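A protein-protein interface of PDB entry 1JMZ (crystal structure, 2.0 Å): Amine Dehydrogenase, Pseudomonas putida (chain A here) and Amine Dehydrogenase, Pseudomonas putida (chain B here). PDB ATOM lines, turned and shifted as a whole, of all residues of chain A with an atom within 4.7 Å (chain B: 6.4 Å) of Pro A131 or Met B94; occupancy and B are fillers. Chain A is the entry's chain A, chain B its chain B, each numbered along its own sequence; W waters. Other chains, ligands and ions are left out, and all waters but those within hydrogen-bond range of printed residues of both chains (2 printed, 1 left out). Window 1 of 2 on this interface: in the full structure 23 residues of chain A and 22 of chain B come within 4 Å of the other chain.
OH of Tyr A135 sits at hydrogen-bond distance from OD1 of Asn B111 (2.9 Å).
The backbone carbonyl oxygen (O) of Val B150 sits at hydrogen-bond distance from the side-chain hydroxyl (OH) of Tyr A135 (2.6 Å).
The backbone carbonyl oxygen of Arg B92 lies within hydrogen-bond range of the backbone NH of Asn B111, 3.0 Å away.
CA of Gly A128 touches OG1 of Thr B113, at 3.4 Å.
Pro A131 touches Met B94.
N of Ser A132 touches CE of Met B94 (3.8 Å).
Met B94 touches Tyr A135 (CG to CE2, 3.7 Å).
Of the printed residues of chain B, Gly A128 touches Thr B113 (3.4 Å).
Of chain B, only Met B94 (3.9 Å) comes within 4 Å of Pro A131.
Of the printed residues of chain B, Ser A132 touches Met B94 (3.8 Å).
Of the printed residues of chain B, Tyr A135 touches Met B94 (3.7 Å), Asn B111 (2.9 Å) and Val B150 (2.6 Å).
Tyr B64 touches none of the printed residues of chain A.
Met B94 touches just these residues of chain A: Pro A131 (3.9 Å), Ser A132 (3.8 Å) and Tyr A135 (3.7 Å).
Printed residues of chain A within 4 Å of Thr B113: Gly A128 (3.4 Å).
Printed residues of chain A within 4 Å of Val B150: Tyr A135 (2.6 Å).
The nearest printed residue of chain A that does not touch Met B94 is Leu A133 (6.2 Å).
The nearest printed residue of chain B that does not touch Gly A128 is Arg B92 (6.1 Å).
Printed residues of chain B that touch a printed residue of chain A: Met B94, Asn B111, Thr B113 and Val B150.
Hydrophobic or aromatic side chains of chain B that line the printed part of chain A: Met B94.
Hydrophobic or aromatic side chains of chain A within 4 Å of the printed part of chain B: Tyr A135.
Water W1 bridges OE2 of Glu A134 (2.8 Å) and OD1 of Asn B111 (3.3 Å).
Water W2 lies within hydrogen-bond range of ND2 of Asn B111 (2.8 Å), N of Val B150 (3.0 Å) and OH of Tyr A135 (3.3 Å).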
ATOM      1  N   LEU A 127      11.234 -26.478 -29.569  1.00  0.00           N
ATOM      2  CA  LEU A 127      10.191 -27.367 -29.070  1.00  0.00           C
ATOM      3  C   LEU A 127       9.478 -26.758 -27.867  1.00  0.00           C
ATOM      4  O   LEU A 127       8.323 -27.068 -27.613  1.00  0.00           O
ATOM      5  CB  LEU A 127      10.768 -28.738 -28.710  1.00  0.00           C
ATOM      6  CG  LEU A 127       9.999 -29.969 -29.192  1.00  0.00           C
ATOM      7  CD1 LEU A 127      10.539 -31.192 -28.509  1.00  0.00           C
ATOM      8  CD2 LEU A 127       8.518 -29.842 -28.931  1.00  0.00           C
ATOM      9  N   GLY A 128      10.167 -25.876 -27.148  1.00  0.00           N
ATOM     10  CA  GLY A 128       9.570 -25.230 -25.989  1.00  0.00           C
ATOM     11  C   GLY A 128       8.669 -24.048 -26.313  1.00  0.00           C
ATOM     12  O   GLY A 128       7.643 -23.838 -25.653  1.00  0.00           O
ATOM     13  N   GLN A 129       9.051 -23.276 -27.331  1.00  0.00           N
ATOM     14  CA  GLN A 129       8.294 -22.102 -27.760  1.00  0.00           C
ATOM     15  C   GLN A 129       7.122 -22.493 -28.670  1.00  0.00           C
ATOM     16  O   GLN A 129       6.081 -21.836 -28.689  1.00  0.00           O
ATOM     17  CB  GLN A 129       9.226 -21.111 -28.474  1.00  0.00           C
ATOM     18  CG  GLN A 129       8.618 -19.731 -28.756  1.00  0.00           C
ATOM     19  CD  GLN A 129       8.349 -18.922 -27.490  1.00  0.00           C
ATOM     20  OE1 GLN A 129       8.923 -19.186 -26.436  1.00  0.00           O
ATOM     21  NE2 GLN A 129       7.470 -17.935 -27.595  1.00  0.00           N
ATOM     22  N   TRP A 130       7.309 -23.568 -29.426  1.00  0.00           N
ATOM     23  CA  TRP A 130       6.282 -24.062 -30.325  1.00  0.00           C
ATOM     24  C   TRP A 130       6.094 -25.556 -30.080  1.00  0.00           C
ATOM     25  O   TRP A 130       6.634 -26.384 -30.806  1.00  0.00           O
ATOM     26  CB  TRP A 130       6.673 -23.796 -31.785  1.00  0.00           C
ATOM     27  CG  TRP A 130       6.895 -22.351 -32.068  1.00  0.00           C
ATOM     28  CD1 TRP A 130       5.954 -21.370 -32.079  1.00  0.00           C
ATOM     29  CD2 TRP A 130       8.159 -21.698 -32.266  1.00  0.00           C
ATOM     30  NE1 TRP A 130       6.548 -20.145 -32.252  1.00  0.00           N
ATOM     31  CE2 TRP A 130       7.900 -20.315 -32.369  1.00  0.00           C
ATOM     32  CE3 TRP A 130       9.483 -22.149 -32.357  1.00  0.00           C
ATOM     33  CZ2 TRP A 130       8.917 -19.374 -32.555  1.00  0.00           C
ATOM     34  CZ3 TRP A 130      10.492 -21.214 -32.541  1.00  0.00           C
ATOM     35  CH2 TRP A 130      10.201 -19.841 -32.637  1.00  0.00           C
ATOM     36  N   PRO A 131       5.334 -25.915 -29.026  1.00  0.00           N
ATOM     37  CA  PRO A 131       5.063 -27.311 -28.661  1.00  0.00           C
ATOM     38  C   PRO A 131       4.504 -28.189 -29.784  1.00  0.00           C
ATOM     39  O   PRO A 131       4.720 -29.397 -29.788  1.00  0.00           O
ATOM     40  CB  PRO A 131       4.074 -27.173 -27.499  1.00  0.00           C
ATOM     41  CG  PRO A 131       4.491 -25.893 -26.853  1.00  0.00           C
ATOM     42  CD  PRO A 131       4.708 -24.998 -28.057  1.00  0.00           C
ATOM     43  N   SER A 132       3.810 -27.578 -30.741  1.00  0.00           N
ATOM     44  CA  SER A 132       3.230 -28.321 -31.855  1.00  0.00           C
ATOM     45  C   SER A 132       4.263 -28.815 -32.869  1.00  0.00           C
ATOM     46  O   SER A 132       3.957 -29.658 -33.709  1.00  0.00           O
ATOM     47  CB  SER A 132       2.189 -27.467 -32.574  1.00  0.00           C
ATOM     48  OG  SER A 132       2.809 -26.369 -33.212  1.00  0.00           O
ATOM     49  N   LEU A 133       5.482 -28.285 -32.786  1.00  0.00           N
ATOM     50  CA  LEU A 133       6.577 -28.644 -33.685  1.00  0.00           C
ATOM     51  C   LEU A 133       6.710 -30.141 -33.984  1.00  0.00           C
ATOM     52  O   LEU A 133       6.785 -30.536 -35.146  1.00  0.00           O
ATOM     53  CB  LEU A 133       7.907 -28.098 -33.127  1.00  0.00           C
ATOM     54  CG  LEU A 133       9.228 -28.173 -33.910  1.00  0.00           C
ATOM     55  CD1 LEU A 133      10.196 -27.144 -33.368  1.00  0.00           C
ATOM     56  CD2 LEU A 133       9.848 -29.556 -33.844  1.00  0.00           C
ATOM     57  N   GLU A 134       6.739 -30.960 -32.932  1.00  0.00           N
ATOM     58  CA  GLU A 134       6.904 -32.411 -33.061  1.00  0.00           C
ATOM     59  C   GLU A 134       5.668 -33.192 -33.509  1.00  0.00           C
ATOM     60  O   GLU A 134       5.704 -34.413 -33.595  1.00  0.00           O
ATOM     61  CB  GLU A 134       7.447 -32.992 -31.750  1.00  0.00           C
ATOM     62  CG  GLU A 134       6.498 -32.842 -30.580  1.00  0.00           C
ATOM     63  CD  GLU A 134       7.106 -33.252 -29.251  1.00  0.00           C
ATOM     64  OE1 GLU A 134       7.982 -34.141 -29.221  1.00  0.00           O
ATOM     65  OE2 GLU A 134       6.693 -32.679 -28.227  1.00  0.00           O
ATOM     66  N   TYR A 135       4.576 -32.485 -33.776  1.00  0.00           N
ATOM     67  CA  TYR A 135       3.337 -33.107 -34.230  1.00  0.00           C
ATOM     68  C   TYR A 135       3.061 -32.724 -35.678  1.00  0.00           C
ATOM     69  O   TYR A 135       2.039 -33.105 -36.236  1.00  0.00           O
ATOM     70  CB  TYR A 135       2.157 -32.641 -33.381  1.00  0.00           C
ATOM     71  CG  TYR A 135       2.203 -33.060 -31.936  1.00  0.00           C
ATOM     72  CD1 TYR A 135       1.506 -34.186 -31.501  1.00  0.00           C
ATOM     73  CD2 TYR A 135       2.907 -32.311 -30.991  1.00  0.00           C
ATOM     74  CE1 TYR A 135       1.501 -34.552 -30.168  1.00  0.00           C
ATOM     75  CE2 TYR A 135       2.909 -32.674 -29.652  1.00  0.00           C
ATOM     76  CZ  TYR A 135       2.201 -33.795 -29.250  1.00  0.00           C
ATOM     77  OH  TYR A 135       2.188 -34.169 -27.937  1.00  0.00           O
ATOM     78  N   LEU B  60     -10.541 -27.421 -23.182  1.00  0.00           N
ATOM     79  CA  LEU B  60      -9.098 -27.176 -23.163  1.00  0.00           C
ATOM     80  C   LEU B  60      -9.049 -25.774 -23.746  1.00  0.00           C
ATOM     81  O   LEU B  60      -9.416 -25.566 -24.897  1.00  0.00           O
ATOM     82  CB  LEU B  60      -8.359 -28.124 -24.108  1.00  0.00           C
ATOM     83  CG  LEU B  60      -6.896 -28.486 -23.822  1.00  0.00           C
ATOM     84  CD1 LEU B  60      -6.167 -28.690 -25.144  1.00  0.00           C
ATOM     85  CD2 LEU B  60      -6.189 -27.450 -22.971  1.00  0.00           C
ATOM     86  N   TYR B  64      -4.015 -23.689 -24.749  1.00  0.00           N
ATOM     87  CA  TYR B  64      -3.606 -25.066 -24.482  1.00  0.00           C
ATOM     88  C   TYR B  64      -2.963 -25.285 -23.111  1.00  0.00           C
ATOM     89  O   TYR B  64      -2.199 -26.228 -22.935  1.00  0.00           O
ATOM     90  CB  TYR B  64      -2.641 -25.541 -25.580  1.00  0.00           C
ATOM     91  CG  TYR B  64      -3.171 -25.405 -27.002  1.00  0.00           C
ATOM     92  CD1 TYR B  64      -3.339 -24.149 -27.596  1.00  0.00           C
ATOM     93  CD2 TYR B  64      -3.517 -26.535 -27.745  1.00  0.00           C
ATOM     94  CE1 TYR B  64      -3.841 -24.024 -28.885  1.00  0.00           C
ATOM     95  CE2 TYR B  64      -4.017 -26.419 -29.038  1.00  0.00           C
ATOM     96  CZ  TYR B  64      -4.181 -25.165 -29.602  1.00  0.00           C
ATOM     97  OH  TYR B  64      -4.704 -25.061 -30.869  1.00  0.00           O
ATOM     98  N   ARG B  92       1.789 -27.512 -21.638  1.00  0.00           N
ATOM     99  CA  ARG B  92       0.857 -27.380 -22.746  1.00  0.00           C
ATOM    100  C   ARG B  92       0.226 -28.723 -23.083  1.00  0.00           C
ATOM    101  O   ARG B  92       0.871 -29.761 -22.993  1.00  0.00           O
ATOM    102  CB  ARG B  92       1.576 -26.849 -23.981  1.00  0.00           C
ATOM    103  CG  ARG B  92       1.197 -25.443 -24.379  1.00  0.00           C
ATOM    104  CD  ARG B  92       1.964 -24.395 -23.607  1.00  0.00           C
ATOM    105  NE  ARG B  92       1.046 -23.428 -23.007  1.00  0.00           N
ATOM    106  CZ  ARG B  92       1.127 -22.104 -23.143  1.00  0.00           C
ATOM    107  NH1 ARG B  92       2.095 -21.550 -23.873  1.00  0.00           N
ATOM    108  NH2 ARG B  92       0.243 -21.333 -22.516  1.00  0.00           N
ATOM    109  N   SER B  93      -1.026 -28.694 -23.510  1.00  0.00           N
ATOM    110  CA  SER B  93      -1.717 -29.912 -23.864  1.00  0.00           C
ATOM    111  C   SER B  93      -2.097 -29.885 -25.349  1.00  0.00           C
ATOM    112  O   SER B  93      -2.878 -29.043 -25.775  1.00  0.00           O
ATOM    113  CB  SER B  93      -2.956 -30.070 -22.987  1.00  0.00           C
ATOM    114  OG  SER B  93      -3.615 -31.289 -23.249  1.00  0.00           O
ATOM    115  N   MET B  94      -1.533 -30.807 -26.127  1.00  0.00           N
ATOM    116  CA  MET B  94      -1.818 -30.882 -27.559  1.00  0.00           C
ATOM    117  C   MET B  94      -3.128 -31.644 -27.771  1.00  0.00           C
ATOM    118  O   MET B  94      -3.126 -32.785 -28.253  1.00  0.00           O
ATOM    119  CB  MET B  94      -0.655 -31.567 -28.293  1.00  0.00           C
ATOM    120  CG  MET B  94      -0.552 -31.251 -29.787  1.00  0.00           C
ATOM    121  SD  MET B  94      -0.363 -29.479 -30.167  1.00  0.00           S
ATOM    122  CE  MET B  94       0.735 -28.949 -28.879  1.00  0.00           C
ATOM    123  N   TYR B  95      -4.238 -30.997 -27.389  1.00  0.00           N
ATOM    124  CA  TYR B  95      -5.589 -31.564 -27.479  1.00  0.00           C
ATOM    125  C   TYR B  95      -5.711 -32.884 -26.699  1.00  0.00           C
ATOM    126  O   TYR B  95      -6.600 -33.682 -26.972  1.00  0.00           O
ATOM    127  CB  TYR B  95      -5.999 -31.792 -28.943  1.00  0.00           C
ATOM    128  CG  TYR B  95      -6.016 -30.547 -29.803  1.00  0.00           C
ATOM    129  CD1 TYR B  95      -4.854 -30.090 -30.424  1.00  0.00           C
ATOM    130  CD2 TYR B  95      -7.194 -29.838 -30.010  1.00  0.00           C
ATOM    131  CE1 TYR B  95      -4.862 -28.954 -31.232  1.00  0.00           C
ATOM    132  CE2 TYR B  95      -7.218 -28.699 -30.824  1.00  0.00           C
ATOM    133  CZ  TYR B  95      -6.046 -28.263 -31.429  1.00  0.00           C
ATOM    134  OH  TYR B  95      -6.048 -27.135 -32.216  1.00  0.00           O
ATOM    135  N   SER B  96      -4.848 -33.075 -25.700  1.00  0.00           N
ATOM    136  CA  SER B  96      -4.826 -34.304 -24.920  1.00  0.00           C
ATOM    137  C   SER B  96      -5.477 -34.219 -23.550  1.00  0.00           C
ATOM    138  O   SER B  96      -4.838 -33.855 -22.576  1.00  0.00           O
ATOM    139  CB  SER B  96      -3.391 -34.825 -24.782  1.00  0.00           C
ATOM    140  N   PHE B  97      -6.751 -34.583 -23.490  1.00  0.00           N
ATOM    141  CA  PHE B  97      -7.524 -34.580 -22.251  1.00  0.00           C
ATOM    142  C   PHE B  97      -8.728 -35.517 -22.418  1.00  0.00           C
ATOM    143  O   PHE B  97      -9.212 -35.725 -23.533  1.00  0.00           O
ATOM    144  CB  PHE B  97      -7.994 -33.158 -21.890  1.00  0.00           C
ATOM    145  N   THR B 109      -2.408 -35.021 -20.761  1.00  0.00           N
ATOM    146  CA  THR B 109      -0.964 -35.192 -20.851  1.00  0.00           C
ATOM    147  C   THR B 109      -0.373 -33.800 -21.079  1.00  0.00           C
ATOM    148  O   THR B 109      -0.907 -32.979 -21.831  1.00  0.00           O
ATOM    149  CB  THR B 109      -0.468 -36.312 -21.833  1.00  0.00           C
ATOM    150  OG1 THR B 109       0.474 -35.785 -22.773  1.00  0.00           O
ATOM    151  CG2 THR B 109      -1.593 -37.006 -22.502  1.00  0.00           C
ATOM    152  N   ASN B 111       2.944 -31.556 -21.835  1.00  0.00           N
ATOM    153  CA  ASN B 111       4.260 -31.492 -22.463  1.00  0.00           C
ATOM    154  C   ASN B 111       4.804 -30.224 -21.811  1.00  0.00           C
ATOM    155  O   ASN B 111       4.410 -29.122 -22.181  1.00  0.00           O
ATOM    156  CB  ASN B 111       4.149 -31.271 -23.981  1.00  0.00           C
ATOM    157  CG  ASN B 111       3.473 -32.425 -24.722  1.00  0.00           C
ATOM    158  OD1 ASN B 111       3.221 -32.318 -25.915  1.00  0.00           O
ATOM    159  ND2 ASN B 111       3.196 -33.521 -24.034  1.00  0.00           N
ATOM    160  N   THR B 113       7.807 -27.417 -20.394  1.00  0.00           N
ATOM    161  CA  THR B 113       9.070 -26.802 -20.746  1.00  0.00           C
ATOM    162  C   THR B 113       9.515 -25.920 -19.598  1.00  0.00           C
ATOM    163  O   THR B 113       8.798 -25.027 -19.162  1.00  0.00           O
ATOM    164  CB  THR B 113       8.985 -25.943 -22.012  1.00  0.00           C
ATOM    165  OG1 THR B 113       8.584 -26.762 -23.112  1.00  0.00           O
ATOM    166  CG2 THR B 113      10.346 -25.314 -22.322  1.00  0.00           C
ATOM    167  N   VAL B 150       2.052 -37.357 -27.863  1.00  0.00           N
ATOM    168  CA  VAL B 150       0.720 -37.820 -27.506  1.00  0.00           C
ATOM    169  C   VAL B 150      -0.279 -36.685 -27.733  1.00  0.00           C
ATOM    170  O   VAL B 150       0.016 -35.521 -27.460  1.00  0.00           O
ATOM    171  CB  VAL B 150       0.672 -38.314 -26.029  1.00  0.00           C
ATOM    172  CG1 VAL B 150      -0.754 -38.371 -25.520  1.00  0.00           C
ATOM    173  CG2 VAL B 150       1.326 -39.692 -25.916  1.00  0.00           C
ATOM    174  N   TYR B 151      -1.436 -37.028 -28.293  1.00  0.00           N
ATOM    175  CA  TYR B 151      -2.498 -36.066 -28.551  1.00  0.00           C
ATOM    176  C   TYR B 151      -3.851 -36.591 -28.036  1.00  0.00           C
ATOM    177  O   TYR B 151      -3.989 -36.808 -26.839  1.00  0.00           O
ATOM    178  CB  TYR B 151      -2.521 -35.641 -30.032  1.00  0.00           C
ATOM    179  CG  TYR B 151      -2.551 -36.761 -31.058  1.00  0.00           C
ATOM    180  CD1 TYR B 151      -3.694 -36.985 -31.835  1.00  0.00           C
ATOM    181  CD2 TYR B 151      -1.443 -37.591 -31.265  1.00  0.00           C
ATOM    182  CE1 TYR B 151      -3.743 -38.005 -32.786  1.00  0.00           C
ATOM    183  CE2 TYR B 151      -1.482 -38.619 -32.221  1.00  0.00           C
ATOM    184  CZ  TYR B 151      -2.644 -38.815 -32.974  1.00  0.00           C
ATOM    185  OH  TYR B 151      -2.725 -39.830 -33.895  1.00  0.00           O
ATOM    186  N   LEU B 152      -4.835 -36.824 -28.904  1.00  0.00           N
ATOM    187  CA  LEU B 152      -6.150 -37.311 -28.467  1.00  0.00           C
ATOM    188  C   LEU B 152      -6.163 -38.520 -27.518  1.00  0.00           C
ATOM    189  O   LEU B 152      -5.361 -39.441 -27.655  1.00  0.00           O
ATOM    190  CB  LEU B 152      -7.035 -37.617 -29.673  1.00  0.00           C
ATOM    191  CG  LEU B 152      -7.410 -36.445 -30.576  1.00  0.00           C
ATOM    192  CD1 LEU B 152      -8.257 -36.963 -31.714  1.00  0.00           C
ATOM    193  CD2 LEU B 152      -8.153 -35.381 -29.803  1.00  0.00           C
ATOM    194  N   PHE B 200      -7.149 -33.802 -34.475  1.00  0.00           N
ATOM    195  CA  PHE B 200      -7.298 -33.032 -33.244  1.00  0.00           C
ATOM    196  C   PHE B 200      -8.768 -32.798 -32.895  1.00  0.00           C
ATOM    197  O   PHE B 200      -9.113 -31.864 -32.181  1.00  0.00           O
ATOM    198  CB  PHE B 200      -6.571 -31.687 -33.381  1.00  0.00           C
ATOM    199  CG  PHE B 200      -5.074 -31.814 -33.446  1.00  0.00           C
ATOM    200  CD1 PHE B 200      -4.402 -32.726 -32.631  1.00  0.00           C
ATOM    201  CD2 PHE B 200      -4.337 -31.043 -34.332  1.00  0.00           C
ATOM    202  CE1 PHE B 200      -3.021 -32.872 -32.700  1.00  0.00           C
ATOM    203  CE2 PHE B 200      -2.950 -31.183 -34.407  1.00  0.00           C
ATOM    204  CZ  PHE B 200      -2.293 -32.106 -33.585  1.00  0.00           C
HETATM  205  O   HOH W   1       5.570 -34.563 -26.498  1.00  0.00           O
HETATM  206  O   HOH W   2       3.100 -36.003 -25.386  1.00  0.00           O
